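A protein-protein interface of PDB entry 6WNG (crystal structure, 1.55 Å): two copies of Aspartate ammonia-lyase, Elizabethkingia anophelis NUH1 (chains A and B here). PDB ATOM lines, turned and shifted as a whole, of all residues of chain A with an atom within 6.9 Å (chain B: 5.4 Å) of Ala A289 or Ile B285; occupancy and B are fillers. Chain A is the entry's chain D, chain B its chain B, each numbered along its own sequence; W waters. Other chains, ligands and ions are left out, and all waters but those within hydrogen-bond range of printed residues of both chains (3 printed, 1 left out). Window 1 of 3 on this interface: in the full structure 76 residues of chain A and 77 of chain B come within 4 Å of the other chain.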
ATOM      1  N   GLU A 220      14.350 -33.699  11.275  1.00  0.00           N
ATOM      2  CA  GLU A 220      14.574 -32.383  11.861  1.00  0.00           C
ATOM      3  C   GLU A 220      14.978 -31.350  10.824  1.00  0.00           C
ATOM      4  O   GLU A 220      14.817 -30.151  11.082  1.00  0.00           O
ATOM      5  CB  GLU A 220      15.639 -32.471  12.957  1.00  0.00           C
ATOM      6  CG  GLU A 220      15.294 -33.524  13.995  1.00  0.00           C
ATOM      7  CD  GLU A 220      13.850 -33.388  14.456  1.00  0.00           C
ATOM      8  OE1 GLU A 220      13.572 -32.454  15.235  1.00  0.00           O
ATOM      9  OE2 GLU A 220      12.998 -34.208  14.028  1.00  0.00           O
ATOM     10  N   ARG A 223      11.911 -29.510   9.827  1.00  0.00           N
ATOM     11  CA  ARG A 223      11.406 -28.684  10.915  1.00  0.00           C
ATOM     12  C   ARG A 223      12.247 -27.423  11.072  1.00  0.00           C
ATOM     13  O   ARG A 223      11.707 -26.320  11.200  1.00  0.00           O
ATOM     14  CB  ARG A 223      11.367 -29.487  12.216  1.00  0.00           C
ATOM     15  CG  ARG A 223      10.617 -30.806  12.109  1.00  0.00           C
ATOM     16  CD  ARG A 223       9.120 -30.673  12.408  1.00  0.00           C
ATOM     17  NE  ARG A 223       8.455 -29.674  11.578  1.00  0.00           N
ATOM     18  CZ  ARG A 223       8.136 -29.844  10.298  1.00  0.00           C
ATOM     19  NH1 ARG A 223       7.527 -28.867   9.636  1.00  0.00           N
ATOM     20  NH2 ARG A 223       8.433 -30.981   9.676  1.00  0.00           N
ATOM     21  N   LEU A 224      13.572 -27.568  11.058  1.00  0.00           N
ATOM     22  CA  LEU A 224      14.427 -26.396  11.192  1.00  0.00           C
ATOM     23  C   LEU A 224      14.258 -25.456  10.004  1.00  0.00           C
ATOM     24  O   LEU A 224      14.130 -24.241  10.185  1.00  0.00           O
ATOM     25  CB  LEU A 224      15.885 -26.830  11.337  1.00  0.00           C
ATOM     26  CG  LEU A 224      16.207 -27.522  12.668  1.00  0.00           C
ATOM     27  CD1 LEU A 224      17.576 -28.210  12.597  1.00  0.00           C
ATOM     28  CD2 LEU A 224      16.179 -26.522  13.834  1.00  0.00           C
ATOM     29  N   ASN A 225      14.221 -26.003   8.788  1.00  0.00           N
ATOM     30  CA  ASN A 225      14.135 -25.153   7.601  1.00  0.00           C
ATOM     31  C   ASN A 225      12.793 -24.436   7.516  1.00  0.00           C
ATOM     32  O   ASN A 225      12.742 -23.233   7.220  1.00  0.00           O
ATOM     33  CB  ASN A 225      14.386 -25.976   6.331  1.00  0.00           C
ATOM     34  CG  ASN A 225      15.855 -26.273   6.116  1.00  0.00           C
ATOM     35  OD1 ASN A 225      16.720 -25.639   6.730  1.00  0.00           O
ATOM     36  ND2 ASN A 225      16.153 -27.242   5.247  1.00  0.00           N
ATOM     37  N   ASN A 227      10.691 -23.667   9.881  1.00  0.00           N
ATOM     38  CA  ASN A 227      10.549 -22.637  10.898  1.00  0.00           C
ATOM     39  C   ASN A 227      11.516 -21.483  10.669  1.00  0.00           C
ATOM     40  O   ASN A 227      11.152 -20.331  10.904  1.00  0.00           O
ATOM     41  CB  ASN A 227      10.709 -23.250  12.289  1.00  0.00           C
ATOM     42  CG  ASN A 227       9.464 -23.996  12.709  1.00  0.00           C
ATOM     43  OD1 ASN A 227       8.426 -23.384  12.944  1.00  0.00           O
ATOM     44  ND2 ASN A 227       9.546 -25.326  12.758  1.00  0.00           N
ATOM     45  N   ALA A 228      12.729 -21.757  10.170  1.00  0.00           N
ATOM     46  CA  ALA A 228      13.616 -20.646   9.821  1.00  0.00           C
ATOM     47  C   ALA A 228      13.055 -19.821   8.668  1.00  0.00           C
ATOM     48  O   ALA A 228      13.321 -18.615   8.583  1.00  0.00           O
ATOM     49  CB  ALA A 228      15.013 -21.160   9.481  1.00  0.00           C
ATOM     50  N   TYR A 283      10.717 -16.407  16.474  1.00  0.00           N
ATOM     51  CA  TYR A 283      11.829 -16.818  17.328  1.00  0.00           C
ATOM     52  C   TYR A 283      11.414 -17.943  18.261  1.00  0.00           C
ATOM     53  O   TYR A 283      12.184 -18.883  18.489  1.00  0.00           O
ATOM     54  CB  TYR A 283      12.351 -15.633  18.151  1.00  0.00           C
ATOM     55  CG  TYR A 283      12.530 -14.368  17.342  1.00  0.00           C
ATOM     56  CD1 TYR A 283      13.430 -14.314  16.281  1.00  0.00           C
ATOM     57  CD2 TYR A 283      11.790 -13.231  17.642  1.00  0.00           C
ATOM     58  CE1 TYR A 283      13.579 -13.154  15.525  1.00  0.00           C
ATOM     59  CE2 TYR A 283      11.920 -12.070  16.895  1.00  0.00           C
ATOM     60  CZ  TYR A 283      12.818 -12.033  15.838  1.00  0.00           C
ATOM     61  OH  TYR A 283      12.934 -10.874  15.095  1.00  0.00           O
ATOM     62  N   VAL A 284      10.205 -17.846  18.827  1.00  0.00           N
ATOM     63  CA  VAL A 284       9.713 -18.855  19.763  1.00  0.00           C
ATOM     64  C   VAL A 284       9.630 -20.216  19.091  1.00  0.00           C
ATOM     65  O   VAL A 284      10.091 -21.220  19.643  1.00  0.00           O
ATOM     66  CB  VAL A 284       8.350 -18.436  20.336  1.00  0.00           C
ATOM     67  CG1 VAL A 284       7.757 -19.547  21.202  1.00  0.00           C
ATOM     68  CG2 VAL A 284       8.499 -17.180  21.155  1.00  0.00           C
ATOM     69  N   ILE A 285       9.036 -20.279  17.896  1.00  0.00           N
ATOM     70  CA  ILE A 285       8.836 -21.601  17.306  1.00  0.00           C
ATOM     71  C   ILE A 285      10.133 -22.116  16.683  1.00  0.00           C
ATOM     72  O   ILE A 285      10.367 -23.335  16.657  1.00  0.00           O
ATOM     73  CB  ILE A 285       7.659 -21.580  16.308  1.00  0.00           C
ATOM     74  CG1 ILE A 285       7.165 -23.007  15.990  1.00  0.00           C
ATOM     75  CG2 ILE A 285       8.039 -20.849  15.028  1.00  0.00           C
ATOM     76  CD1 ILE A 285       6.467 -23.691  17.154  1.00  0.00           C
ATOM     77  N   TYR A 286      11.013 -21.230  16.201  1.00  0.00           N
ATOM     78  CA  TYR A 286      12.323 -21.699  15.749  1.00  0.00           C
ATOM     79  C   TYR A 286      13.131 -22.276  16.909  1.00  0.00           C
ATOM     80  O   TYR A 286      13.733 -23.355  16.786  1.00  0.00           O
ATOM     81  CB  TYR A 286      13.121 -20.586  15.047  1.00  0.00           C
ATOM     82  CG  TYR A 286      14.454 -21.138  14.567  1.00  0.00           C
ATOM     83  CD1 TYR A 286      14.513 -21.972  13.452  1.00  0.00           C
ATOM     84  CD2 TYR A 286      15.637 -20.887  15.267  1.00  0.00           C
ATOM     85  CE1 TYR A 286      15.714 -22.534  13.031  1.00  0.00           C
ATOM     86  CE2 TYR A 286      16.848 -21.440  14.854  1.00  0.00           C
ATOM     87  CZ  TYR A 286      16.879 -22.268  13.742  1.00  0.00           C
ATOM     88  OH  TYR A 286      18.069 -22.823  13.327  1.00  0.00           O
ATOM     89  N   SER A 287      13.165 -21.567  18.043  1.00  0.00           N
ATOM     90  CA  SER A 287      13.833 -22.103  19.225  1.00  0.00           C
ATOM     91  C   SER A 287      13.215 -23.434  19.643  1.00  0.00           C
ATOM     92  O   SER A 287      13.929 -24.348  20.075  1.00  0.00           O
ATOM     93  CB  SER A 287      13.776 -21.073  20.362  1.00  0.00           C
ATOM     94  OG  SER A 287      14.472 -21.524  21.521  1.00  0.00           O
ATOM     95  N   SER A 288      11.892 -23.570  19.498  1.00  0.00           N
ATOM     96  CA  SER A 288      11.223 -24.830  19.823  1.00  0.00           C
ATOM     97  C   SER A 288      11.656 -25.948  18.886  1.00  0.00           C
ATOM     98  O   SER A 288      11.758 -27.111  19.309  1.00  0.00           O
ATOM     99  CB  SER A 288       9.710 -24.655  19.756  1.00  0.00           C
ATOM    100  OG  SER A 288       9.260 -23.750  20.748  1.00  0.00           O
ATOM    101  N   ALA A 289      11.906 -25.625  17.610  1.00  0.00           N
ATOM    102  CA  ALA A 289      12.404 -26.645  16.691  1.00  0.00           C
ATOM    103  C   ALA A 289      13.807 -27.087  17.080  1.00  0.00           C
ATOM    104  O   ALA A 289      14.123 -28.284  17.013  1.00  0.00           O
ATOM    105  CB  ALA A 289      12.383 -26.127  15.248  1.00  0.00           C
ATOM    106  N   MET A 290      14.661 -26.147  17.505  1.00  0.00           N
ATOM    107  CA  MET A 290      15.958 -26.552  18.038  1.00  0.00           C
ATOM    108  C   MET A 290      15.795 -27.412  19.281  1.00  0.00           C
ATOM    109  O   MET A 290      16.526 -28.393  19.458  1.00  0.00           O
ATOM    110  CB  MET A 290      16.826 -25.334  18.358  1.00  0.00           C
ATOM    111  CG  MET A 290      17.256 -24.555  17.150  1.00  0.00           C
ATOM    112  SD  MET A 290      18.626 -23.455  17.602  1.00  0.00           S
ATOM    113  CE  MET A 290      17.808 -22.305  18.673  1.00  0.00           C
ATOM    114  N   LYS A 291      14.843 -27.058  20.152  1.00  0.00           N
ATOM    115  CA  LYS A 291      14.599 -27.847  21.354  1.00  0.00           C
ATOM    116  C   LYS A 291      14.172 -29.262  21.002  1.00  0.00           C
ATOM    117  O   LYS A 291      14.651 -30.227  21.605  1.00  0.00           O
ATOM    118  CB  LYS A 291      13.532 -27.170  22.221  1.00  0.00           C
ATOM    119  CG  LYS A 291      13.252 -27.937  23.523  1.00  0.00           C
ATOM    120  CD  LYS A 291      11.992 -27.436  24.213  1.00  0.00           C
ATOM    121  CE  LYS A 291      10.735 -28.020  23.581  1.00  0.00           C
ATOM    122  NZ  LYS A 291       9.533 -27.524  24.315  1.00  0.00           N
ATOM    123  N   ARG A 292      13.271 -29.406  20.026  1.00  0.00           N
ATOM    124  CA  ARG A 292      12.843 -30.741  19.608  1.00  0.00           C
ATOM    125  C   ARG A 292      14.026 -31.564  19.112  1.00  0.00           C
ATOM    126  O   ARG A 292      14.165 -32.745  19.461  1.00  0.00           O
ATOM    127  CB  ARG A 292      11.768 -30.634  18.524  1.00  0.00           C
ATOM    128  CG  ARG A 292      11.499 -31.955  17.798  1.00  0.00           C
ATOM    129  CD  ARG A 292      10.428 -31.815  16.713  1.00  0.00           C
ATOM    130  NE  ARG A 292      10.751 -32.658  15.564  1.00  0.00           N
ATOM    131  CZ  ARG A 292       9.867 -33.185  14.720  1.00  0.00           C
ATOM    132  NH1 ARG A 292       8.567 -33.003  14.899  1.00  0.00           N
ATOM    133  NH2 ARG A 292      10.296 -33.903  13.679  1.00  0.00           N
ATOM    134  N   MET A 293      14.902 -30.959  18.307  1.00  0.00           N
ATOM    135  CA  MET A 293      16.061 -31.704  17.826  1.00  0.00           C
ATOM    136  C   MET A 293      16.987 -32.073  18.978  1.00  0.00           C
ATOM    137  O   MET A 293      17.515 -33.194  19.026  1.00  0.00           O
ATOM    138  CB  MET A 293      16.822 -30.902  16.769  1.00  0.00           C
ATOM    139  CG  MET A 293      18.085 -31.633  16.302  1.00  0.00           C
ATOM    140  SD  MET A 293      18.978 -30.774  14.999  1.00  0.00           S
ATOM    141  CE  MET A 293      19.432 -29.259  15.835  1.00  0.00           C
ATOM    142  N   ALA A 294      17.175 -31.155  19.931  1.00  0.00           N
ATOM    143  CA  ALA A 294      18.035 -31.432  21.080  1.00  0.00           C
ATOM    144  C   ALA A 294      17.475 -32.576  21.915  1.00  0.00           C
ATOM    145  O   ALA A 294      18.230 -33.412  22.426  1.00  0.00           O
ATOM    146  CB  ALA A 294      18.193 -30.174  21.936  1.00  0.00           C
ATOM    147  N   ASP A 353      15.851 -22.258  25.595  1.00  0.00           N
ATOM    148  CA  ASP A 353      14.521 -22.138  25.011  1.00  0.00           C
ATOM    149  C   ASP A 353      13.521 -21.557  26.013  1.00  0.00           C
ATOM    150  O   ASP A 353      12.602 -20.817  25.619  1.00  0.00           O
ATOM    151  CB  ASP A 353      14.074 -23.507  24.485  1.00  0.00           C
ATOM    152  CG  ASP A 353      12.691 -23.469  23.879  1.00  0.00           C
ATOM    153  OD1 ASP A 353      12.527 -22.860  22.792  1.00  0.00           O
ATOM    154  OD2 ASP A 353      11.759 -24.007  24.513  1.00  0.00           O
ATOM    155  N   ASN B 227       1.749 -28.119  12.141  1.00  0.00           N
ATOM    156  CA  ASN B 227       2.332 -29.036  13.110  1.00  0.00           C
ATOM    157  C   ASN B 227       1.391 -30.195  13.430  1.00  0.00           C
ATOM    158  O   ASN B 227       1.855 -31.324  13.600  1.00  0.00           O
ATOM    159  CB  ASN B 227       2.761 -28.260  14.360  1.00  0.00           C
ATOM    160  CG  ASN B 227       4.042 -27.490  14.111  1.00  0.00           C
ATOM    161  OD1 ASN B 227       5.100 -28.088  13.942  1.00  0.00           O
ATOM    162  ND2 ASN B 227       3.945 -26.165  14.030  1.00  0.00           N
ATOM    163  N   LEU B 230       1.677 -33.168  11.128  1.00  0.00           N
ATOM    164  CA  LEU B 230       2.728 -34.147  11.399  1.00  0.00           C
ATOM    165  C   LEU B 230       2.169 -35.405  12.046  1.00  0.00           C
ATOM    166  O   LEU B 230       2.760 -36.481  11.911  1.00  0.00           O
ATOM    167  CB  LEU B 230       3.805 -33.527  12.290  1.00  0.00           C
ATOM    168  CG  LEU B 230       4.493 -32.300  11.690  1.00  0.00           C
ATOM    169  CD1 LEU B 230       5.414 -31.680  12.730  1.00  0.00           C
ATOM    170  CD2 LEU B 230       5.277 -32.659  10.426  1.00  0.00           C
ATOM    171  N   GLY B 281       8.596 -36.753  18.466  1.00  0.00           N
ATOM    172  CA  GLY B 281       8.882 -35.396  18.007  1.00  0.00           C
ATOM    173  C   GLY B 281       7.656 -34.596  17.591  1.00  0.00           C
ATOM    174  O   GLY B 281       7.611 -33.372  17.779  1.00  0.00           O
ATOM    175  N   ALA B 282       6.656 -35.255  16.991  1.00  0.00           N
ATOM    176  CA  ALA B 282       5.476 -34.511  16.547  1.00  0.00           C
ATOM    177  C   ALA B 282       4.740 -33.896  17.734  1.00  0.00           C
ATOM    178  O   ALA B 282       4.274 -32.753  17.657  1.00  0.00           O
ATOM    179  CB  ALA B 282       4.537 -35.414  15.743  1.00  0.00           C
ATOM    180  N   TYR B 283       4.651 -34.628  18.849  1.00  0.00           N
ATOM    181  CA  TYR B 283       3.989 -34.093  20.040  1.00  0.00           C
ATOM    182  C   TYR B 283       4.751 -32.900  20.593  1.00  0.00           C
ATOM    183  O   TYR B 283       4.143 -31.911  21.035  1.00  0.00           O
ATOM    184  CB  TYR B 283       3.852 -35.169  21.133  1.00  0.00           C
ATOM    185  CG  TYR B 283       3.428 -36.524  20.610  1.00  0.00           C
ATOM    186  CD1 TYR B 283       2.182 -36.704  20.025  1.00  0.00           C
ATOM    187  CD2 TYR B 283       4.276 -37.623  20.710  1.00  0.00           C
ATOM    188  CE1 TYR B 283       1.793 -37.934  19.517  1.00  0.00           C
ATOM    189  CE2 TYR B 283       3.894 -38.864  20.217  1.00  0.00           C
ATOM    190  CZ  TYR B 283       2.647 -39.012  19.622  1.00  0.00           C
ATOM    191  OH  TYR B 283       2.254 -40.240  19.111  1.00  0.00           O
ATOM    192  N   VAL B 284       6.086 -32.970  20.568  1.00  0.00           N
ATOM    193  CA  VAL B 284       6.897 -31.882  21.109  1.00  0.00           C
ATOM    194  C   VAL B 284       6.662 -30.603  20.318  1.00  0.00           C
ATOM    195  O   VAL B 284       6.432 -29.534  20.893  1.00  0.00           O
ATOM    196  CB  VAL B 284       8.387 -32.273  21.119  1.00  0.00           C
ATOM    197  CG1 VAL B 284       9.253 -31.093  21.536  1.00  0.00           C
ATOM    198  CG2 VAL B 284       8.602 -33.422  22.062  1.00  0.00           C
ATOM    199  N   ILE B 285       6.714 -30.689  18.987  1.00  0.00           N
ATOM    200  CA  ILE B 285       6.616 -29.447  18.226  1.00  0.00           C
ATOM    201  C   ILE B 285       5.163 -28.953  18.160  1.00  0.00           C
ATOM    202  O   ILE B 285       4.929 -27.741  18.120  1.00  0.00           O
ATOM    203  CB  ILE B 285       7.261 -29.606  16.833  1.00  0.00           C
ATOM    204  CG1 ILE B 285       7.511 -28.231  16.205  1.00  0.00           C
ATOM    205  CG2 ILE B 285       6.410 -30.463  15.907  1.00  0.00           C
ATOM    206  CD1 ILE B 285       8.570 -27.411  16.934  1.00  0.00           C
ATOM    207  N   TYR B 286       4.168 -29.855  18.197  1.00  0.00           N
ATOM    208  CA  TYR B 286       2.786 -29.382  18.272  1.00  0.00           C
ATOM    209  C   TYR B 286       2.516 -28.686  19.598  1.00  0.00           C
ATOM    210  O   TYR B 286       1.896 -27.612  19.630  1.00  0.00           O
ATOM    211  CB  TYR B 286       1.783 -30.529  18.065  1.00  0.00           C
ATOM    212  CG  TYR B 286       0.367 -30.010  18.152  1.00  0.00           C
ATOM    213  CD1 TYR B 286      -0.175 -29.268  17.112  1.00  0.00           C
ATOM    214  CD2 TYR B 286      -0.401 -30.205  19.299  1.00  0.00           C
ATOM    215  CE1 TYR B 286      -1.469 -28.750  17.192  1.00  0.00           C
ATOM    216  CE2 TYR B 286      -1.684 -29.695  19.395  1.00  0.00           C
ATOM    217  CZ  TYR B 286      -2.213 -28.969  18.340  1.00  0.00           C
ATOM    218  OH  TYR B 286      -3.491 -28.449  18.451  1.00  0.00           O
ATOM    219  N   SER B 287       2.971 -29.282  20.707  1.00  0.00           N
ATOM    220  CA  SER B 287       2.839 -28.617  22.002  1.00  0.00           C
ATOM    221  C   SER B 287       3.524 -27.250  21.985  1.00  0.00           C
ATOM    222  O   SER B 287       2.998 -26.270  22.534  1.00  0.00           O
ATOM    223  CB  SER B 287       3.414 -29.509  23.111  1.00  0.00           C
ATOM    224  OG  SER B 287       3.239 -28.902  24.384  1.00  0.00           O
ATOM    225  N   SER B 288       4.682 -27.157  21.321  1.00  0.00           N
ATOM    226  CA  SER B 288       5.386 -25.884  21.207  1.00  0.00           C
ATOM    227  C   SER B 288       4.574 -24.859  20.426  1.00  0.00           C
ATOM    228  O   SER B 288       4.611 -23.664  20.744  1.00  0.00           O
ATOM    229  CB  SER B 288       6.741 -26.096  20.538  1.00  0.00           C
ATOM    230  OG  SER B 288       7.591 -26.882  21.360  1.00  0.00           O
ATOM    231  N   ALA B 289       3.857 -25.302  19.384  1.00  0.00           N
ATOM    232  CA  ALA B 289       2.988 -24.392  18.647  1.00  0.00           C
ATOM    233  C   ALA B 289       1.853 -23.880  19.527  1.00  0.00           C
ATOM    234  O   ALA B 289       1.500 -22.697  19.462  1.00  0.00           O
ATOM    235  CB  ALA B 289       2.453 -25.089  17.393  1.00  0.00           C
ATOM    236  N   MET B 290       1.276 -24.742  20.370  1.00  0.00           N
ATOM    237  CA  MET B 290       0.294 -24.256  21.336  1.00  0.00           C
ATOM    238  C   MET B 290       0.928 -23.266  22.296  1.00  0.00           C
ATOM    239  O   MET B 290       0.308 -22.260  22.657  1.00  0.00           O
ATOM    240  CB  MET B 290      -0.323 -25.415  22.121  1.00  0.00           C
ATOM    241  CG  MET B 290      -1.236 -26.290  21.313  1.00  0.00           C
ATOM    242  SD  MET B 290      -2.256 -27.296  22.427  1.00  0.00           S
ATOM    243  CE  MET B 290      -1.004 -28.293  23.208  1.00  0.00           C
HETATM  244  O   HOH W   1       5.891 -24.344  12.565  1.00  0.00           O
HETATM  245  O   HOH W   2       7.216 -27.293  12.478  1.00  0.00           O
HETATM  246  O   HOH W   3       7.345 -29.239  23.915  1.00  0.00           O
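Ile A285 touches Ser B288, and with the chains exchanged Ser A288 touches Ile B285.
Ile A285 touches Ala B289, and with the chains exchanged Ala A289 touches Ile B285.
Ser B288 touches its own counterpart, Ser A288.
9 positions are printed for both chains.
Of the 12 pairs that touch across the chains among the printed residues, 5 have their exchanged pair printed and touching as well.
Among the printed residues, merely in contact across the chains: Arg A223 with Leu B230, Ile A285 with Ser B288, Ile A285 with Ala B289, Ser A288 with Ile B285, Ser A288 with Ser B288, Ala A289 with Ile B285, Lys A291 with Val B284, Lys A291 with Ser B288, Arg A292 with Ala B282, Arg A292 with Val B284 and Arg A292 with Ile B285.
Of the 19 printed residues of chain A, 6 touch a printed residue of chain B.
Hydrophobic or aromatic side chains of chain A within 4 Å of the printed part of chain B: Ile A285.
Hydrophobic or aromatic side chains of chain B within 4 Å of the printed part of chain A: Leu B230, Val B284 and Ile B285.
Among the printed residues, 12 pairs touch across the chains.
Among the printed residues, no Asp or Glu carboxylate lies within 4 Å of a Lys or Arg side-chain nitrogen of the other chain.
O of Val B284 sits at hydrogen-bond distance from OG of Ser B288 (2.9 Å).
The guanidinium group of Arg A292 lies within salt-bridge range of the side-chain carboxylate of Glu A220 (2.7 Å).
The side-chain amide nitrogen (ND2) of Asn A227 lies within hydrogen-bond range of the backbone carbonyl oxygen (O) of Arg A223, at 2.8 Å.
The backbone carbonyl oxygen of Val A284 lies within hydrogen-bond range of the side-chain hydroxyl of Ser A288 (2.9 Å).
The side-chain carboxylate (OD1) of Asp A353 is in hydrogen-bond range of the backbone NH (N) of Ser A288 (3.4 Å).
Water W2 lies within hydrogen-bond range of OD1 of Asn B227 (2.7 Å), NE of Arg A223 (2.8 Å) and ND2 of Asn A227 (3.1 Å).
Water W1 lies within hydrogen-bond range of the side-chain amide oxygen (OD1) of Asn A227 (2.7 Å) and the side-chain amide nitrogen (ND2) of Asn B227 (3.0 Å).
Water W3 lies within hydrogen-bond range of NZ of Lys A291 (2.8 Å), O of Val B284 (3.2 Å) and OG of Ser B288 (3.5 Å).
The guanidinium group (NH1) of Arg A292 lies within hydrogen-bond range of the backbone carbonyl oxygen (O) of Gly B281, 3.1 Å away.
Ala A289 touches just one residue of chain B: Ile B285 (3.8 Å).
Of the printed residues of chain A, Leu B230 touches Arg A223 (3.7 Å).
Of the printed residues of chain A, Ala B282 touches Arg A292.
Ile B285 touches just these residues of chain A: Ser A288 (3.9 Å), Ala A289 (3.8 Å) and Arg A292 (3.5 Å).
The nearest printed residue of chain B that does not touch Ala A289 is Ser B288 (5.9 Å).
The nearest residue of chain A that does not touch Ile B285 is Ile A285 (4.3 Å).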
